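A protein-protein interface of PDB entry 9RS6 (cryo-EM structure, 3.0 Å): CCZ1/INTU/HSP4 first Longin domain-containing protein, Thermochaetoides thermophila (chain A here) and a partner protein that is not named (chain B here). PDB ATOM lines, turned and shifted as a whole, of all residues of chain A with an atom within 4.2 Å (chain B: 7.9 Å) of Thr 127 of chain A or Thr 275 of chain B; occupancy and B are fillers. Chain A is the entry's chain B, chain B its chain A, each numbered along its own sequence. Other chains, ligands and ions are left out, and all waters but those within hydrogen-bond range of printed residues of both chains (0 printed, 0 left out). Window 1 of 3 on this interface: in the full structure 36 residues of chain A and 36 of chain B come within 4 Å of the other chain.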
ATOM      1  N   VAL A 125       2.607  -7.338   0.954  1.00  0.00           N
ATOM      2  CA  VAL A 125       2.323  -6.871  -0.400  1.00  0.00           C
ATOM      3  C   VAL A 125       0.832  -7.050  -0.663  1.00  0.00           C
ATOM      4  O   VAL A 125       0.352  -8.175  -0.827  1.00  0.00           O
ATOM      5  CB  VAL A 125       3.164  -7.619  -1.438  1.00  0.00           C
ATOM      6  CG1 VAL A 125       2.935  -7.035  -2.815  1.00  0.00           C
ATOM      7  CG2 VAL A 125       4.628  -7.545  -1.072  1.00  0.00           C
ATOM      8  N   ASP A 126       0.095  -5.939  -0.698  1.00  0.00           N
ATOM      9  CA  ASP A 126      -1.343  -6.019  -0.919  1.00  0.00           C
ATOM     10  C   ASP A 126      -1.664  -6.437  -2.347  1.00  0.00           C
ATOM     11  O   ASP A 126      -2.462  -7.356  -2.566  1.00  0.00           O
ATOM     12  CB  ASP A 126      -1.992  -4.673  -0.600  1.00  0.00           C
ATOM     13  CG  ASP A 126      -1.926  -4.330   0.874  1.00  0.00           C
ATOM     14  OD1 ASP A 126      -1.900  -5.263   1.703  1.00  0.00           O
ATOM     15  OD2 ASP A 126      -1.901  -3.126   1.202  1.00  0.00           O
ATOM     16  N   THR A 127      -1.053  -5.779  -3.331  1.00  0.00           N
ATOM     17  CA  THR A 127      -1.372  -6.014  -4.731  1.00  0.00           C
ATOM     18  C   THR A 127      -0.079  -6.165  -5.514  1.00  0.00           C
ATOM     19  O   THR A 127       0.980  -5.704  -5.087  1.00  0.00           O
ATOM     20  CB  THR A 127      -2.205  -4.871  -5.328  1.00  0.00           C
ATOM     21  OG1 THR A 127      -1.436  -3.662  -5.312  1.00  0.00           O
ATOM     22  CG2 THR A 127      -3.475  -4.651  -4.522  1.00  0.00           C
ATOM     23  N   ILE A 128      -0.175  -6.826  -6.665  1.00  0.00           N
ATOM     24  CA  ILE A 128       0.926  -6.992  -7.604  1.00  0.00           C
ATOM     25  C   ILE A 128       0.375  -6.663  -8.985  1.00  0.00           C
ATOM     26  O   ILE A 128      -0.583  -7.300  -9.447  1.00  0.00           O
ATOM     27  CB  ILE A 128       1.516  -8.410  -7.577  1.00  0.00           C
ATOM     28  CG1 ILE A 128       2.179  -8.714  -6.229  1.00  0.00           C
ATOM     29  CG2 ILE A 128       2.498  -8.602  -8.715  1.00  0.00           C
ATOM     30  CD1 ILE A 128       1.267  -9.371  -5.212  1.00  0.00           C
ATOM     31  N   VAL A 135      -2.485  -9.465 -10.017  1.00  0.00           N
ATOM     32  CA  VAL A 135      -2.437 -10.375  -8.881  1.00  0.00           C
ATOM     33  C   VAL A 135      -2.747  -9.587  -7.616  1.00  0.00           C
ATOM     34  O   VAL A 135      -2.366  -8.421  -7.491  1.00  0.00           O
ATOM     35  CB  VAL A 135      -1.064 -11.058  -8.791  1.00  0.00           C
ATOM     36  CG1 VAL A 135      -1.110 -12.224  -7.824  1.00  0.00           C
ATOM     37  CG2 VAL A 135      -0.614 -11.518 -10.167  1.00  0.00           C
ATOM     38  N   PRO A 194      -8.180  -3.793  -7.834  1.00  0.00           N
ATOM     39  CA  PRO A 194      -7.707  -4.717  -6.791  1.00  0.00           C
ATOM     40  C   PRO A 194      -8.329  -4.481  -5.426  1.00  0.00           C
ATOM     41  O   PRO A 194      -8.430  -5.428  -4.638  1.00  0.00           O
ATOM     42  CB  PRO A 194      -6.193  -4.473  -6.773  1.00  0.00           C
ATOM     43  CG  PRO A 194      -6.001  -3.138  -7.409  1.00  0.00           C
ATOM     44  CD  PRO A 194      -7.079  -3.024  -8.434  1.00  0.00           C
ATOM     45  N   TYR B 264       9.372 -13.912 -12.534  1.00  0.00           N
ATOM     46  CA  TYR B 264       8.323 -13.377 -13.400  1.00  0.00           C
ATOM     47  C   TYR B 264       8.715 -13.427 -14.873  1.00  0.00           C
ATOM     48  O   TYR B 264       7.875 -13.724 -15.726  1.00  0.00           O
ATOM     49  CB  TYR B 264       7.941 -11.958 -12.983  1.00  0.00           C
ATOM     50  CG  TYR B 264       7.081 -11.907 -11.748  1.00  0.00           C
ATOM     51  CD1 TYR B 264       6.455 -13.053 -11.283  1.00  0.00           C
ATOM     52  CD2 TYR B 264       6.850 -10.714 -11.080  1.00  0.00           C
ATOM     53  CE1 TYR B 264       5.653 -13.024 -10.175  1.00  0.00           C
ATOM     54  CE2 TYR B 264       6.044 -10.673  -9.969  1.00  0.00           C
ATOM     55  CZ  TYR B 264       5.448 -11.830  -9.515  1.00  0.00           C
ATOM     56  OH  TYR B 264       4.637 -11.830  -8.408  1.00  0.00           O
ATOM     57  N   LEU B 271       6.888  -7.785 -14.533  1.00  0.00           N
ATOM     58  CA  LEU B 271       6.305  -7.099 -13.388  1.00  0.00           C
ATOM     59  C   LEU B 271       6.279  -5.598 -13.648  1.00  0.00           C
ATOM     60  O   LEU B 271       7.226  -5.042 -14.213  1.00  0.00           O
ATOM     61  CB  LEU B 271       7.096  -7.405 -12.116  1.00  0.00           C
ATOM     62  CG  LEU B 271       6.624  -6.742 -10.820  1.00  0.00           C
ATOM     63  CD1 LEU B 271       5.152  -7.005 -10.607  1.00  0.00           C
ATOM     64  CD2 LEU B 271       7.414  -7.248  -9.630  1.00  0.00           C
ATOM     65  N   GLY B 273       5.170  -3.558 -10.911  1.00  0.00           N
ATOM     66  CA  GLY B 273       5.166  -2.999  -9.574  1.00  0.00           C
ATOM     67  C   GLY B 273       4.187  -3.716  -8.666  1.00  0.00           C
ATOM     68  O   GLY B 273       3.342  -4.498  -9.097  1.00  0.00           O
ATOM     69  N   PHE B 274       4.324  -3.426  -7.375  1.00  0.00           N
ATOM     70  CA  PHE B 274       3.470  -4.028  -6.364  1.00  0.00           C
ATOM     71  C   PHE B 274       3.392  -3.096  -5.163  1.00  0.00           C
ATOM     72  O   PHE B 274       4.354  -2.399  -4.837  1.00  0.00           O
ATOM     73  CB  PHE B 274       3.975  -5.418  -5.948  1.00  0.00           C
ATOM     74  CG  PHE B 274       5.438  -5.471  -5.610  1.00  0.00           C
ATOM     75  CD1 PHE B 274       6.388  -5.645  -6.601  1.00  0.00           C
ATOM     76  CD2 PHE B 274       5.861  -5.383  -4.295  1.00  0.00           C
ATOM     77  CE1 PHE B 274       7.732  -5.705  -6.292  1.00  0.00           C
ATOM     78  CE2 PHE B 274       7.203  -5.448  -3.979  1.00  0.00           C
ATOM     79  CZ  PHE B 274       8.139  -5.607  -4.979  1.00  0.00           C
ATOM     80  N   THR B 275       2.235  -3.092  -4.512  1.00  0.00           N
ATOM     81  CA  THR B 275       1.957  -2.177  -3.416  1.00  0.00           C
ATOM     82  C   THR B 275       1.869  -2.936  -2.100  1.00  0.00           C
ATOM     83  O   THR B 275       1.167  -3.947  -2.001  1.00  0.00           O
ATOM     84  CB  THR B 275       0.652  -1.412  -3.658  1.00  0.00           C
ATOM     85  OG1 THR B 275       0.643  -0.889  -4.992  1.00  0.00           O
ATOM     86  CG2 THR B 275       0.513  -0.266  -2.669  1.00  0.00           C
ATOM     87  N   ALA B 276       2.588  -2.445  -1.093  1.00  0.00           N
ATOM     88  CA  ALA B 276       2.526  -2.966   0.268  1.00  0.00           C
ATOM     89  C   ALA B 276       2.031  -1.825   1.153  1.00  0.00           C
ATOM     90  O   ALA B 276       2.826  -1.046   1.687  1.00  0.00           O
ATOM     91  CB  ALA B 276       3.878  -3.499   0.725  1.00  0.00           C
ATOM     92  N   GLY B 277       0.714  -1.722   1.282  1.00  0.00           N
ATOM     93  CA  GLY B 277       0.121  -0.712   2.143  1.00  0.00           C
ATOM     94  C   GLY B 277       0.487   0.688   1.697  1.00  0.00           C
ATOM     95  O   GLY B 277       0.083   1.156   0.626  1.00  0.00           O
ATOM     96  N   LYS B 278       1.273   1.373   2.529  1.00  0.00           N
ATOM     97  CA  LYS B 278       1.663   2.744   2.230  1.00  0.00           C
ATOM     98  C   LYS B 278       2.811   2.825   1.234  1.00  0.00           C
ATOM     99  O   LYS B 278       3.017   3.890   0.641  1.00  0.00           O
ATOM    100  CB  LYS B 278       2.044   3.473   3.519  1.00  0.00           C
ATOM    101  CG  LYS B 278       3.267   2.902   4.215  1.00  0.00           C
ATOM    102  CD  LYS B 278       3.555   3.634   5.515  1.00  0.00           C
ATOM    103  CE  LYS B 278       4.794   3.080   6.198  1.00  0.00           C
ATOM    104  NZ  LYS B 278       4.585   1.686   6.678  1.00  0.00           N
ATOM    105  N   VAL B 279       3.562   1.743   1.027  1.00  0.00           N
ATOM    106  CA  VAL B 279       4.725   1.796   0.149  1.00  0.00           C
ATOM    107  C   VAL B 279       4.358   1.175  -1.192  1.00  0.00           C
ATOM    108  O   VAL B 279       3.511   0.279  -1.280  1.00  0.00           O
ATOM    109  CB  VAL B 279       5.956   1.110   0.788  1.00  0.00           C
ATOM    110  CG1 VAL B 279       5.802  -0.396   0.820  1.00  0.00           C
ATOM    111  CG2 VAL B 279       7.232   1.506   0.067  1.00  0.00           C
ATOM    112  N   ARG B 280       4.971   1.685  -2.257  1.00  0.00           N
ATOM    113  CA  ARG B 280       4.700   1.201  -3.602  1.00  0.00           C
ATOM    114  C   ARG B 280       6.010   1.010  -4.351  1.00  0.00           C
ATOM    115  O   ARG B 280       6.879   1.885  -4.327  1.00  0.00           O
ATOM    116  CB  ARG B 280       3.789   2.169  -4.369  1.00  0.00           C
ATOM    117  CG  ARG B 280       3.884   2.057  -5.880  1.00  0.00           C
ATOM    118  CD  ARG B 280       3.351   3.303  -6.559  1.00  0.00           C
ATOM    119  NE  ARG B 280       2.049   3.695  -6.035  1.00  0.00           N
ATOM    120  CZ  ARG B 280       0.895   3.170  -6.422  1.00  0.00           C
ATOM    121  NH1 ARG B 280       0.842   2.223  -7.345  1.00  0.00           N
ATOM    122  NH2 ARG B 280      -0.234   3.605  -5.870  1.00  0.00           N
ATOM    123  N   PHE B 281       6.144  -0.136  -5.015  1.00  0.00           N
ATOM    124  CA  PHE B 281       7.314  -0.472  -5.812  1.00  0.00           C
ATOM    125  C   PHE B 281       6.905  -0.413  -7.275  1.00  0.00           C
ATOM    126  O   PHE B 281       5.935  -1.063  -7.675  1.00  0.00           O
ATOM    127  CB  PHE B 281       7.847  -1.866  -5.464  1.00  0.00           C
ATOM    128  CG  PHE B 281       8.156  -2.074  -3.998  1.00  0.00           C
ATOM    129  CD1 PHE B 281       7.144  -2.194  -3.055  1.00  0.00           C
ATOM    130  CD2 PHE B 281       9.468  -2.190  -3.572  1.00  0.00           C
ATOM    131  CE1 PHE B 281       7.437  -2.397  -1.721  1.00  0.00           C
ATOM    132  CE2 PHE B 281       9.766  -2.394  -2.239  1.00  0.00           C
ATOM    133  CZ  PHE B 281       8.749  -2.497  -1.313  1.00  0.00           C
ATOM    134  N   VAL B 282       7.628   0.369  -8.069  1.00  0.00           N
ATOM    135  CA  VAL B 282       7.352   0.502  -9.495  1.00  0.00           C
ATOM    136  C   VAL B 282       8.614   0.114 -10.244  1.00  0.00           C
ATOM    137  O   VAL B 282       9.678   0.697 -10.013  1.00  0.00           O
ATOM    138  CB  VAL B 282       6.908   1.928  -9.856  1.00  0.00           C
ATOM    139  CG1 VAL B 282       7.050   2.175 -11.347  1.00  0.00           C
ATOM    140  CG2 VAL B 282       5.482   2.165  -9.400  1.00  0.00           C
ATOM    141  N   SER B 295       8.418   4.066  -3.186  1.00  0.00           N
ATOM    142  CA  SER B 295       7.878   5.331  -2.712  1.00  0.00           C
ATOM    143  C   SER B 295       7.001   5.116  -1.490  1.00  0.00           C
ATOM    144  O   SER B 295       6.120   4.249  -1.495  1.00  0.00           O
ATOM    145  CB  SER B 295       7.073   6.027  -3.808  1.00  0.00           C
ATOM    146  OG  SER B 295       6.232   7.023  -3.254  1.00  0.00           O
ATOM    147  N   GLU B 299       2.516   8.201  -3.949  1.00  0.00           N
ATOM    148  CA  GLU B 299       2.674   8.554  -5.350  1.00  0.00           C
ATOM    149  C   GLU B 299       2.151   7.434  -6.239  1.00  0.00           C
ATOM    150  O   GLU B 299       2.221   6.255  -5.889  1.00  0.00           O
ATOM    151  CB  GLU B 299       4.140   8.838  -5.672  1.00  0.00           C
ATOM    152  CG  GLU B 299       4.848   9.611  -4.581  1.00  0.00           C
ATOM    153  CD  GLU B 299       6.267   9.976  -4.949  1.00  0.00           C
ATOM    154  OE1 GLU B 299       6.519  10.272  -6.135  1.00  0.00           O
ATOM    155  OE2 GLU B 299       7.129   9.970  -4.049  1.00  0.00           O
ATOM    156  N   ASP B 301       1.574   5.086  -9.818  1.00  0.00           N
ATOM    157  CA  ASP B 301       2.439   4.323 -10.709  1.00  0.00           C
ATOM    158  C   ASP B 301       2.955   5.199 -11.845  1.00  0.00           C
ATOM    159  O   ASP B 301       4.112   5.072 -12.262  1.00  0.00           O
ATOM    160  CB  ASP B 301       1.666   3.116 -11.251  1.00  0.00           C
ATOM    161  CG  ASP B 301       2.547   2.118 -11.988  1.00  0.00           C
ATOM    162  OD1 ASP B 301       3.766   2.344 -12.120  1.00  0.00           O
ATOM    163  OD2 ASP B 301       2.008   1.086 -12.441  1.00  0.00           O
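The backbone carbonyl oxygen of Thr 275 of chain B is in hydrogen-bond range of the backbone NH of Asp 126 of chain A, at 2.6 Å. The backbone NH of Thr 275 of chain B lies within hydrogen-bond range of the backbone carbonyl oxygen of Thr 127 of chain A (3.0 Å). N of Gly 277 of chain B lies within hydrogen-bond range of OD2 of Asp 126 of chain A (3.0 Å).
The backbone carbonyl oxygen (O) of Phe 281 of chain B lies within hydrogen-bond range of the backbone NH (N) of Phe 274 of chain B, at 2.9 Å. O of Val 135 of chain A is in hydrogen-bond range of N of Ile 128 of chain A, at 2.8 Å.
Among the printed residues, merely in contact across the chains: Thr 127 of chain A with Phe 274 of chain B, Val 125 of chain A with Thr 275 of chain B, Ile 128 of chain A with Leu 271 of chain B, Val 125 of chain A with Phe 274 of chain B, Ile 128 of chain A with Gly 273 of chain B, Ile 128 of chain A with Phe 274 of chain B, Val 125 of chain A with Ala 276 of chain B, Ile 128 of chain A with Tyr 264 of chain B and Asp 126 of chain A with Ala 276 of chain B.
Of chain B, only Phe 274 and Thr 275 come within 4 Å of Thr 127 of chain A. Printed residues of chain B within 4 Å of Ile 128 of chain A: Tyr 264, Leu 271, Gly 273 and Phe 274. Of the printed residues of chain A, Leu 271 of chain B touches Ile 128. Of the printed residues of chain A, Gly 273 of chain B touches Ile 128 (3.7 Å). The nearest residue of chain B that does not touch Thr 127 of chain A is Gly 273 of chain B (4.8 Å). The nearest printed residue of chain B that does not touch Ile 128 of chain A is Thr 275 of chain B (4.9 Å).
Of the 15 printed residues of chain B, 7 touch a printed residue of chain A. Printed residues of chain A that touch a printed residue of chain B: Val 125, Asp 126, Thr 127 and Ile 128. Hydrophobic or aromatic side chains of chain A within 4 Å of the printed part of chain B: Val 125 and Ile 128.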
